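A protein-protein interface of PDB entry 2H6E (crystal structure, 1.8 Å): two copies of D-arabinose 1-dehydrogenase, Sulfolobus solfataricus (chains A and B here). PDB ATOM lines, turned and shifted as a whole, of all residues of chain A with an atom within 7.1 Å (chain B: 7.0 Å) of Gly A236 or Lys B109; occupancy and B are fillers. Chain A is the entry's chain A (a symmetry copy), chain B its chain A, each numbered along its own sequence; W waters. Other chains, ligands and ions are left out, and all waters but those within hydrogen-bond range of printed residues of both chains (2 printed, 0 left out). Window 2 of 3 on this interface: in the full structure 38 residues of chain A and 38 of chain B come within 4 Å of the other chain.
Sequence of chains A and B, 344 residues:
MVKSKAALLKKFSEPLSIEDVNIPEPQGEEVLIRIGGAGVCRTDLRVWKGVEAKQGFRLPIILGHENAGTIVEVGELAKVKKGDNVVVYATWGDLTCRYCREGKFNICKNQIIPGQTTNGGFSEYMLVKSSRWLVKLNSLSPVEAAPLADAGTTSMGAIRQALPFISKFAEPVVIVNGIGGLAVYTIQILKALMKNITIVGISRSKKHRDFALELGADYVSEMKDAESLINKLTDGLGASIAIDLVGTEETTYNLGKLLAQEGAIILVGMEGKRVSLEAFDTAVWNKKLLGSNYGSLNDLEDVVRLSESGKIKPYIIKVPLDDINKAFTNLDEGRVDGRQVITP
The backbone carbonyl oxygen (O) of Gln A261 is in hydrogen-bond range of the side-chain hydroxyl (OH) of Tyr B99, at 2.8 Å. The side-chain amide nitrogen of Gln A261 sits at hydrogen-bond distance from the backbone carbonyl oxygen of Ile B107 (2.9 Å). O of Gly A236 is in hydrogen-bond range of NZ of Lys B109 (2.8 Å).
The side-chain sulfur of Cys B97 lies close to the backbone NH of Tyr B99 (3.5 Å). N of Lys B104 lies within hydrogen-bond range of O of Tyr B99. SG of Cys B108 lies close to N of Asn B110. The backbone NH of Gly A236 lies within hydrogen-bond range of the backbone carbonyl oxygen of Asn A231. The backbone NH of Leu A237 is in hydrogen-bond range of the side-chain hydroxyl of Thr A234 (3.2 Å). The backbone NH (N) of Ala A260 sits at hydrogen-bond distance from the backbone carbonyl oxygen (O) of Ala A239, 2.8 Å away.
Among the printed residues, pairs that only touch across the chains: Ala A260 with Tyr B99, Trp A285 with Ile B107, Trp A285 with Cys B108, Trp A285 with Lys B109, Leu A237 with Tyr B99 and Gln A261 with Lys B109.
Of chain B, only Lys B109 (2.8 Å) comes within 4 Å of Gly A236. Printed residues of chain B within 4 Å of Gln A261: Tyr B99 (2.8 Å), Ile B107 (2.9 Å) and Lys B109 (3.9 Å). Of the printed residues of chain B, Trp A285 touches Ile B107 (3.5 Å), Cys B108 (3.6 Å) and Lys B109 (3.7 Å). Printed residues of chain A within 4 Å of Cys B108: Trp A285. Gly A238 touches none of the printed residues of chain B. The nearest printed residue of chain B that does not touch Gly A236 is Tyr B99 (8.1 Å). The nearest residue of chain A that does not touch Lys B109 is Leu A237 (4.3 Å).
Of the 14 printed residues of chain A, 5 touch a printed residue of chain B. Printed residues of chain A that touch a printed residue of chain B: Gly A236, Leu A237, Ala A260, Gln A261 and Trp A285. Hydrophobic or aromatic side chains of chain A within 4 Å of the printed part of chain B: Leu A237, Ala A260 and Trp A285. Of the 13 printed residues of chain B, 4 touch a printed residue of chain A. Hydrophobic or aromatic side chains of chain B within 4 Å of the printed part of chain A: Tyr B99. Along chain B the printed residues that touch a printed residue of chain A span positions 99 to 109.
No position is printed for both chains. Of the 9 pairs that touch across the chains among the printed residues, none has its exchanged pair printed and touching as well.
Water W2 lies within hydrogen-bond range of O of Leu A237 (2.6 Å), OE1 of Gln A261 (2.7 Å) and NZ of Lys B109 (2.9 Å). Water W1 bridges the backbone NH (N) of Lys B109 (3.1 Å) and the side-chain amide nitrogen (NE2) of Gln A261 (3.3 Å).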
ATOM      1  N   ILE A 230      29.439  22.921   4.528  1.00  0.00           N
ATOM      2  CA  ILE A 230      28.534  23.987   4.138  1.00  0.00           C
ATOM      3  C   ILE A 230      27.960  24.709   5.358  1.00  0.00           C
ATOM      4  O   ILE A 230      27.816  25.958   5.360  1.00  0.00           O
ATOM      5  CB  ILE A 230      27.467  23.477   3.145  1.00  0.00           C
ATOM      6  CG1 ILE A 230      28.155  23.089   1.820  1.00  0.00           C
ATOM      7  CG2 ILE A 230      26.431  24.544   2.891  1.00  0.00           C
ATOM      8  CD1 ILE A 230      27.216  22.543   0.748  1.00  0.00           C
ATOM      9  N   ASN A 231      27.651  23.944   6.401  1.00  0.00           N
ATOM     10  CA  ASN A 231      27.246  24.539   7.672  1.00  0.00           C
ATOM     11  C   ASN A 231      28.269  25.552   8.177  1.00  0.00           C
ATOM     12  O   ASN A 231      27.894  26.637   8.628  1.00  0.00           O
ATOM     13  CB  ASN A 231      27.000  23.459   8.748  1.00  0.00           C
ATOM     14  CG  ASN A 231      25.622  22.810   8.632  1.00  0.00           C
ATOM     15  OD1 ASN A 231      24.762  23.260   7.876  1.00  0.00           O
ATOM     16  ND2 ASN A 231      25.417  21.742   9.387  1.00  0.00           N
ATOM     17  N   LYS A 232      29.550  25.193   8.112  1.00  0.00           N
ATOM     18  CA  LYS A 232      30.610  26.076   8.580  1.00  0.00           C
ATOM     19  C   LYS A 232      30.770  27.299   7.684  1.00  0.00           C
ATOM     20  O   LYS A 232      30.967  28.402   8.187  1.00  0.00           O
ATOM     21  CB  LYS A 232      31.937  25.324   8.705  1.00  0.00           C
ATOM     22  CG  LYS A 232      31.931  24.272   9.822  1.00  0.00           C
ATOM     23  N   LEU A 233      30.640  27.101   6.372  1.00  0.00           N
ATOM     24  CA  LEU A 233      30.819  28.172   5.396  1.00  0.00           C
ATOM     25  C   LEU A 233      29.669  29.178   5.422  1.00  0.00           C
ATOM     26  O   LEU A 233      29.870  30.347   5.102  1.00  0.00           O
ATOM     27  CB  LEU A 233      30.967  27.605   3.981  1.00  0.00           C
ATOM     28  CG  LEU A 233      32.192  26.736   3.692  1.00  0.00           C
ATOM     29  CD1 LEU A 233      32.138  26.253   2.248  1.00  0.00           C
ATOM     30  CD2 LEU A 233      33.478  27.491   3.945  1.00  0.00           C
ATOM     31  N   THR A 234      28.488  28.722   5.822  1.00  0.00           N
ATOM     32  CA  THR A 234      27.275  29.546   5.762  1.00  0.00           C
ATOM     33  C   THR A 234      26.597  29.835   7.113  1.00  0.00           C
ATOM     34  O   THR A 234      25.480  30.308   7.130  1.00  0.00           O
ATOM     35  CB  THR A 234      26.228  28.890   4.818  1.00  0.00           C
ATOM     36  OG1 THR A 234      25.747  27.659   5.386  1.00  0.00           O
ATOM     37  CG2 THR A 234      26.806  28.644   3.427  1.00  0.00           C
ATOM     38  N   ASP A 235      27.284  29.546   8.217  1.00  0.00           N
ATOM     39  CA  ASP A 235      26.705  29.658   9.560  1.00  0.00           C
ATOM     40  C   ASP A 235      25.344  28.969   9.646  1.00  0.00           C
ATOM     41  O   ASP A 235      24.375  29.504  10.199  1.00  0.00           O
ATOM     42  CB  ASP A 235      26.615  31.124   9.982  1.00  0.00           C
ATOM     43  CG  ASP A 235      27.967  31.807   9.980  1.00  0.00           C
ATOM     44  OD1 ASP A 235      28.930  31.202  10.493  1.00  0.00           O
ATOM     45  OD2 ASP A 235      28.071  32.936   9.456  1.00  0.00           O
ATOM     46  N   GLY A 236      25.282  27.774   9.073  1.00  0.00           N
ATOM     47  CA  GLY A 236      24.093  26.939   9.117  1.00  0.00           C
ATOM     48  C   GLY A 236      22.996  27.281   8.135  1.00  0.00           C
ATOM     49  O   GLY A 236      21.959  26.629   8.139  1.00  0.00           O
ATOM     50  N   LEU A 237      23.203  28.285   7.286  1.00  0.00           N
ATOM     51  CA  LEU A 237      22.138  28.709   6.372  1.00  0.00           C
ATOM     52  C   LEU A 237      21.880  27.650   5.317  1.00  0.00           C
ATOM     53  O   LEU A 237      20.737  27.327   5.039  1.00  0.00           O
ATOM     54  CB  LEU A 237      22.495  30.036   5.712  1.00  0.00           C
ATOM     55  CG  LEU A 237      21.536  30.576   4.643  1.00  0.00           C
ATOM     56  CD1 LEU A 237      20.109  30.766   5.203  1.00  0.00           C
ATOM     57  CD2 LEU A 237      22.120  31.893   4.100  1.00  0.00           C
ATOM     58  N   GLY A 238      22.958  27.100   4.751  1.00  0.00           N
ATOM     59  CA  GLY A 238      22.887  26.192   3.626  1.00  0.00           C
ATOM     60  C   GLY A 238      23.266  26.842   2.295  1.00  0.00           C
ATOM     61  O   GLY A 238      23.470  28.053   2.213  1.00  0.00           O
ATOM     62  N   ALA A 239      23.311  26.019   1.251  1.00  0.00           N
ATOM     63  CA  ALA A 239      23.724  26.431  -0.088  1.00  0.00           C
ATOM     64  C   ALA A 239      22.571  27.139  -0.801  1.00  0.00           C
ATOM     65  O   ALA A 239      21.425  26.806  -0.572  1.00  0.00           O
ATOM     66  CB  ALA A 239      24.198  25.223  -0.897  1.00  0.00           C
ATOM     67  N   LEU A 259      20.612  22.500   0.744  1.00  0.00           N
ATOM     68  CA  LEU A 259      20.122  23.801   0.328  1.00  0.00           C
ATOM     69  C   LEU A 259      19.517  24.563   1.483  1.00  0.00           C
ATOM     70  O   LEU A 259      18.936  23.965   2.400  1.00  0.00           O
ATOM     71  CB  LEU A 259      19.059  23.660  -0.763  1.00  0.00           C
ATOM     72  CG  LEU A 259      19.447  22.987  -2.075  1.00  0.00           C
ATOM     73  CD1 LEU A 259      18.198  22.772  -2.913  1.00  0.00           C
ATOM     74  CD2 LEU A 259      20.442  23.836  -2.850  1.00  0.00           C
ATOM     75  N   ALA A 260      19.671  25.885   1.428  1.00  0.00           N
ATOM     76  CA  ALA A 260      18.938  26.800   2.264  1.00  0.00           C
ATOM     77  C   ALA A 260      17.463  26.731   1.863  1.00  0.00           C
ATOM     78  O   ALA A 260      17.133  26.242   0.773  1.00  0.00           O
ATOM     79  CB  ALA A 260      19.486  28.255   2.072  1.00  0.00           C
ATOM     80  N   GLN A 261      16.577  27.180   2.742  1.00  0.00           N
ATOM     81  CA  GLN A 261      15.168  27.360   2.367  1.00  0.00           C
ATOM     82  C   GLN A 261      15.059  28.171   1.075  1.00  0.00           C
ATOM     83  O   GLN A 261      15.834  29.109   0.847  1.00  0.00           O
ATOM     84  CB  GLN A 261      14.342  28.068   3.440  1.00  0.00           C
ATOM     85  CG  GLN A 261      14.363  27.452   4.849  1.00  0.00           C
ATOM     86  CD  GLN A 261      15.420  28.086   5.727  1.00  0.00           C
ATOM     87  OE1 GLN A 261      16.618  27.987   5.433  1.00  0.00           O
ATOM     88  NE2 GLN A 261      14.995  28.731   6.823  1.00  0.00           N
ATOM     89  N   TRP A 285      10.384  23.452   3.462  1.00  0.00           N
ATOM     90  CA  TRP A 285      11.346  24.559   3.297  1.00  0.00           C
ATOM     91  C   TRP A 285      11.286  25.202   1.899  1.00  0.00           C
ATOM     92  O   TRP A 285      12.127  26.030   1.529  1.00  0.00           O
ATOM     93  CB  TRP A 285      12.779  24.098   3.665  1.00  0.00           C
ATOM     94  CG  TRP A 285      12.861  23.469   5.030  1.00  0.00           C
ATOM     95  CD1 TRP A 285      13.277  22.199   5.322  1.00  0.00           C
ATOM     96  CD2 TRP A 285      12.435  24.046   6.288  1.00  0.00           C
ATOM     97  NE1 TRP A 285      13.178  21.960   6.678  1.00  0.00           N
ATOM     98  CE2 TRP A 285      12.664  23.076   7.289  1.00  0.00           C
ATOM     99  CE3 TRP A 285      11.918  25.296   6.666  1.00  0.00           C
ATOM    100  CZ2 TRP A 285      12.370  23.302   8.636  1.00  0.00           C
ATOM    101  CZ3 TRP A 285      11.625  25.522   8.006  1.00  0.00           C
ATOM    102  CH2 TRP A 285      11.845  24.518   8.977  1.00  0.00           C
ATOM    103  N   GLN B  55      10.727  21.367  15.125  1.00  0.00           N
ATOM    104  CA  GLN B  55      11.607  21.830  16.199  1.00  0.00           C
ATOM    105  C   GLN B  55      10.780  22.414  17.341  1.00  0.00           C
ATOM    106  O   GLN B  55       9.850  23.166  17.094  1.00  0.00           O
ATOM    107  CB  GLN B  55      12.575  22.895  15.685  1.00  0.00           C
ATOM    108  CG  GLN B  55      13.748  23.143  16.627  1.00  0.00           C
ATOM    109  CD  GLN B  55      14.717  24.176  16.093  1.00  0.00           C
ATOM    110  OE1 GLN B  55      14.309  25.231  15.607  1.00  0.00           O
ATOM    111  NE2 GLN B  55      16.010  23.884  16.196  1.00  0.00           N
ATOM    112  N   ASP B  94      10.650  33.702  14.088  1.00  0.00           N
ATOM    113  CA  ASP B  94      11.509  34.305  15.109  1.00  0.00           C
ATOM    114  C   ASP B  94      11.772  35.799  14.899  1.00  0.00           C
ATOM    115  O   ASP B  94      12.353  36.449  15.773  1.00  0.00           O
ATOM    116  CB  ASP B  94      12.861  33.562  15.236  1.00  0.00           C
ATOM    117  CG  ASP B  94      13.666  33.547  13.967  1.00  0.00           C
ATOM    118  OD1 ASP B  94      13.324  34.275  13.001  1.00  0.00           O
ATOM    119  OD2 ASP B  94      14.651  32.777  13.927  1.00  0.00           O
ATOM    120  N   CYS B  97      15.467  36.259  11.325  1.00  0.00           N
ATOM    121  CA  CYS B  97      16.201  35.612  10.276  1.00  0.00           C
ATOM    122  C   CYS B  97      15.905  36.271   8.940  1.00  0.00           C
ATOM    123  O   CYS B  97      14.969  37.083   8.813  1.00  0.00           O
ATOM    124  CB  CYS B  97      15.855  34.110  10.248  1.00  0.00           C
ATOM    125  SG  CYS B  97      14.307  33.684   9.459  1.00  0.00           S
ATOM    126  N   TYR B  99      14.568  35.099   6.321  1.00  0.00           N
ATOM    127  CA  TYR B  99      13.268  34.731   5.776  1.00  0.00           C
ATOM    128  C   TYR B  99      12.159  35.560   6.424  1.00  0.00           C
ATOM    129  O   TYR B  99      11.269  36.103   5.723  1.00  0.00           O
ATOM    130  CB  TYR B  99      13.058  33.221   5.894  1.00  0.00           C
ATOM    131  CG  TYR B  99      14.095  32.498   5.084  1.00  0.00           C
ATOM    132  CD1 TYR B  99      13.968  32.371   3.702  1.00  0.00           C
ATOM    133  CD2 TYR B  99      15.235  32.008   5.674  1.00  0.00           C
ATOM    134  CE1 TYR B  99      14.943  31.737   2.945  1.00  0.00           C
ATOM    135  CE2 TYR B  99      16.229  31.383   4.935  1.00  0.00           C
ATOM    136  CZ  TYR B  99      16.076  31.236   3.568  1.00  0.00           C
ATOM    137  OH  TYR B  99      17.046  30.608   2.839  1.00  0.00           O
ATOM    138  N   CYS B 100      12.212  35.705   7.738  1.00  0.00           N
ATOM    139  CA  CYS B 100      11.233  36.555   8.435  1.00  0.00           C
ATOM    140  C   CYS B 100      11.335  38.016   7.979  1.00  0.00           C
ATOM    141  O   CYS B 100      10.325  38.741   7.926  1.00  0.00           O
ATOM    142  CB  CYS B 100      11.439  36.459   9.944  1.00  0.00           C
ATOM    143  SG  CYS B 100      10.882  34.861  10.652  1.00  0.00           S
ATOM    144  N   LYS B 104       8.516  35.841   5.226  1.00  0.00           N
ATOM    145  CA  LYS B 104       8.442  34.410   4.927  1.00  0.00           C
ATOM    146  C   LYS B 104       8.504  33.609   6.233  1.00  0.00           C
ATOM    147  O   LYS B 104       9.309  32.672   6.413  1.00  0.00           O
ATOM    148  CB  LYS B 104       9.490  33.986   3.897  1.00  0.00           C
ATOM    149  CG  LYS B 104       9.337  34.691   2.575  1.00  0.00           C
ATOM    150  CD  LYS B 104      10.486  34.395   1.647  1.00  0.00           C
ATOM    151  CE  LYS B 104      10.464  35.233   0.390  1.00  0.00           C
ATOM    152  NZ  LYS B 104      11.730  35.031  -0.384  1.00  0.00           N
ATOM    153  N   PHE B 105       7.606  33.988   7.139  1.00  0.00           N
ATOM    154  CA  PHE B 105       7.531  33.360   8.484  1.00  0.00           C
ATOM    155  C   PHE B 105       7.297  31.853   8.388  1.00  0.00           C
ATOM    156  O   PHE B 105       7.700  31.063   9.258  1.00  0.00           O
ATOM    157  CB  PHE B 105       6.416  34.014   9.284  1.00  0.00           C
ATOM    158  CG  PHE B 105       6.500  35.521   9.320  1.00  0.00           C
ATOM    159  CD1 PHE B 105       7.552  36.148   9.992  1.00  0.00           C
ATOM    160  CD2 PHE B 105       5.530  36.311   8.692  1.00  0.00           C
ATOM    161  CE1 PHE B 105       7.658  37.549  10.056  1.00  0.00           C
ATOM    162  CE2 PHE B 105       5.611  37.733   8.742  1.00  0.00           C
ATOM    163  CZ  PHE B 105       6.675  38.354   9.410  1.00  0.00           C
ATOM    164  N   ASN B 106       6.626  31.471   7.315  1.00  0.00           N
ATOM    165  CA  ASN B 106       6.242  30.082   7.072  1.00  0.00           C
ATOM    166  C   ASN B 106       7.434  29.141   6.825  1.00  0.00           C
ATOM    167  O   ASN B 106       7.298  27.912   6.958  1.00  0.00           O
ATOM    168  CB  ASN B 106       5.232  30.021   5.914  1.00  0.00           C
ATOM    169  CG  ASN B 106       5.695  30.768   4.685  1.00  0.00           C
ATOM    170  OD1 ASN B 106       6.116  31.926   4.769  1.00  0.00           O
ATOM    171  ND2 ASN B 106       5.595  30.127   3.520  1.00  0.00           N
ATOM    172  N   ILE B 107       8.593  29.702   6.481  1.00  0.00           N
ATOM    173  CA  ILE B 107       9.776  28.873   6.224  1.00  0.00           C
ATOM    174  C   ILE B 107      10.929  29.213   7.169  1.00  0.00           C
ATOM    175  O   ILE B 107      12.080  28.837   6.932  1.00  0.00           O
ATOM    176  CB  ILE B 107      10.201  28.875   4.738  1.00  0.00           C
ATOM    177  CG1 ILE B 107      10.330  30.300   4.209  1.00  0.00           C
ATOM    178  CG2 ILE B 107       9.196  28.053   3.875  1.00  0.00           C
ATOM    179  CD1 ILE B 107      10.876  30.389   2.781  1.00  0.00           C
ATOM    180  N   CYS B 108      10.583  29.865   8.281  1.00  0.00           N
ATOM    181  CA  CYS B 108      11.519  30.116   9.363  1.00  0.00           C
ATOM    182  C   CYS B 108      11.831  28.798  10.059  1.00  0.00           C
ATOM    183  O   CYS B 108      10.918  28.062  10.438  1.00  0.00           O
ATOM    184  CB  CYS B 108      10.930  31.114  10.356  1.00  0.00           C
ATOM    185  SG  CYS B 108      12.013  31.453  11.779  1.00  0.00           S
ATOM    186  N   LYS B 109      13.115  28.509  10.261  1.00  0.00           N
ATOM    187  CA  LYS B 109      13.487  27.228  10.847  1.00  0.00           C
ATOM    188  C   LYS B 109      13.384  27.214  12.382  1.00  0.00           C
ATOM    189  O   LYS B 109      13.597  26.176  13.000  1.00  0.00           O
ATOM    190  CB  LYS B 109      14.848  26.772  10.344  1.00  0.00           C
ATOM    191  CG  LYS B 109      16.048  27.577  10.765  1.00  0.00           C
ATOM    192  CD  LYS B 109      17.229  27.153   9.939  1.00  0.00           C
ATOM    193  CE  LYS B 109      18.492  27.905  10.330  1.00  0.00           C
ATOM    194  NZ  LYS B 109      19.676  27.340   9.616  1.00  0.00           N
ATOM    195  N   ASN B 110      13.063  28.362  12.971  1.00  0.00           N
ATOM    196  CA  ASN B 110      12.824  28.472  14.421  1.00  0.00           C
ATOM    197  C   ASN B 110      11.425  29.021  14.698  1.00  0.00           C
ATOM    198  O   ASN B 110      11.196  29.830  15.618  1.00  0.00           O
ATOM    199  CB  ASN B 110      13.886  29.346  15.065  1.00  0.00           C
ATOM    200  CG  ASN B 110      15.239  28.666  15.135  1.00  0.00           C
ATOM    201  OD1 ASN B 110      15.481  27.852  16.024  1.00  0.00           O
ATOM    202  ND2 ASN B 110      16.135  29.007  14.205  1.00  0.00           N
ATOM    203  N   GLN B 111      10.479  28.566  13.884  1.00  0.00           N
ATOM    204  CA  GLN B 111       9.091  28.984  14.015  1.00  0.00           C
ATOM    205  C   GLN B 111       8.452  28.283  15.225  1.00  0.00           C
ATOM    206  O   GLN B 111       8.871  27.179  15.625  1.00  0.00           O
ATOM    207  CB  GLN B 111       8.351  28.735  12.663  1.00  0.00           C
ATOM    208  CG  GLN B 111       8.031  27.316  12.344  1.00  0.00           C
ATOM    209  CD  GLN B 111       7.744  27.067  10.859  1.00  0.00           C
ATOM    210  OE1 GLN B 111       7.482  27.984  10.091  1.00  0.00           O
ATOM    211  NE2 GLN B 111       7.798  25.813  10.462  1.00  0.00           N
HETATM  212  O   HOH W   1      15.237  30.647   9.546  1.00  0.00           O
HETATM  213  O   HOH W   2      18.831  27.587   6.857  1.00  0.00           O
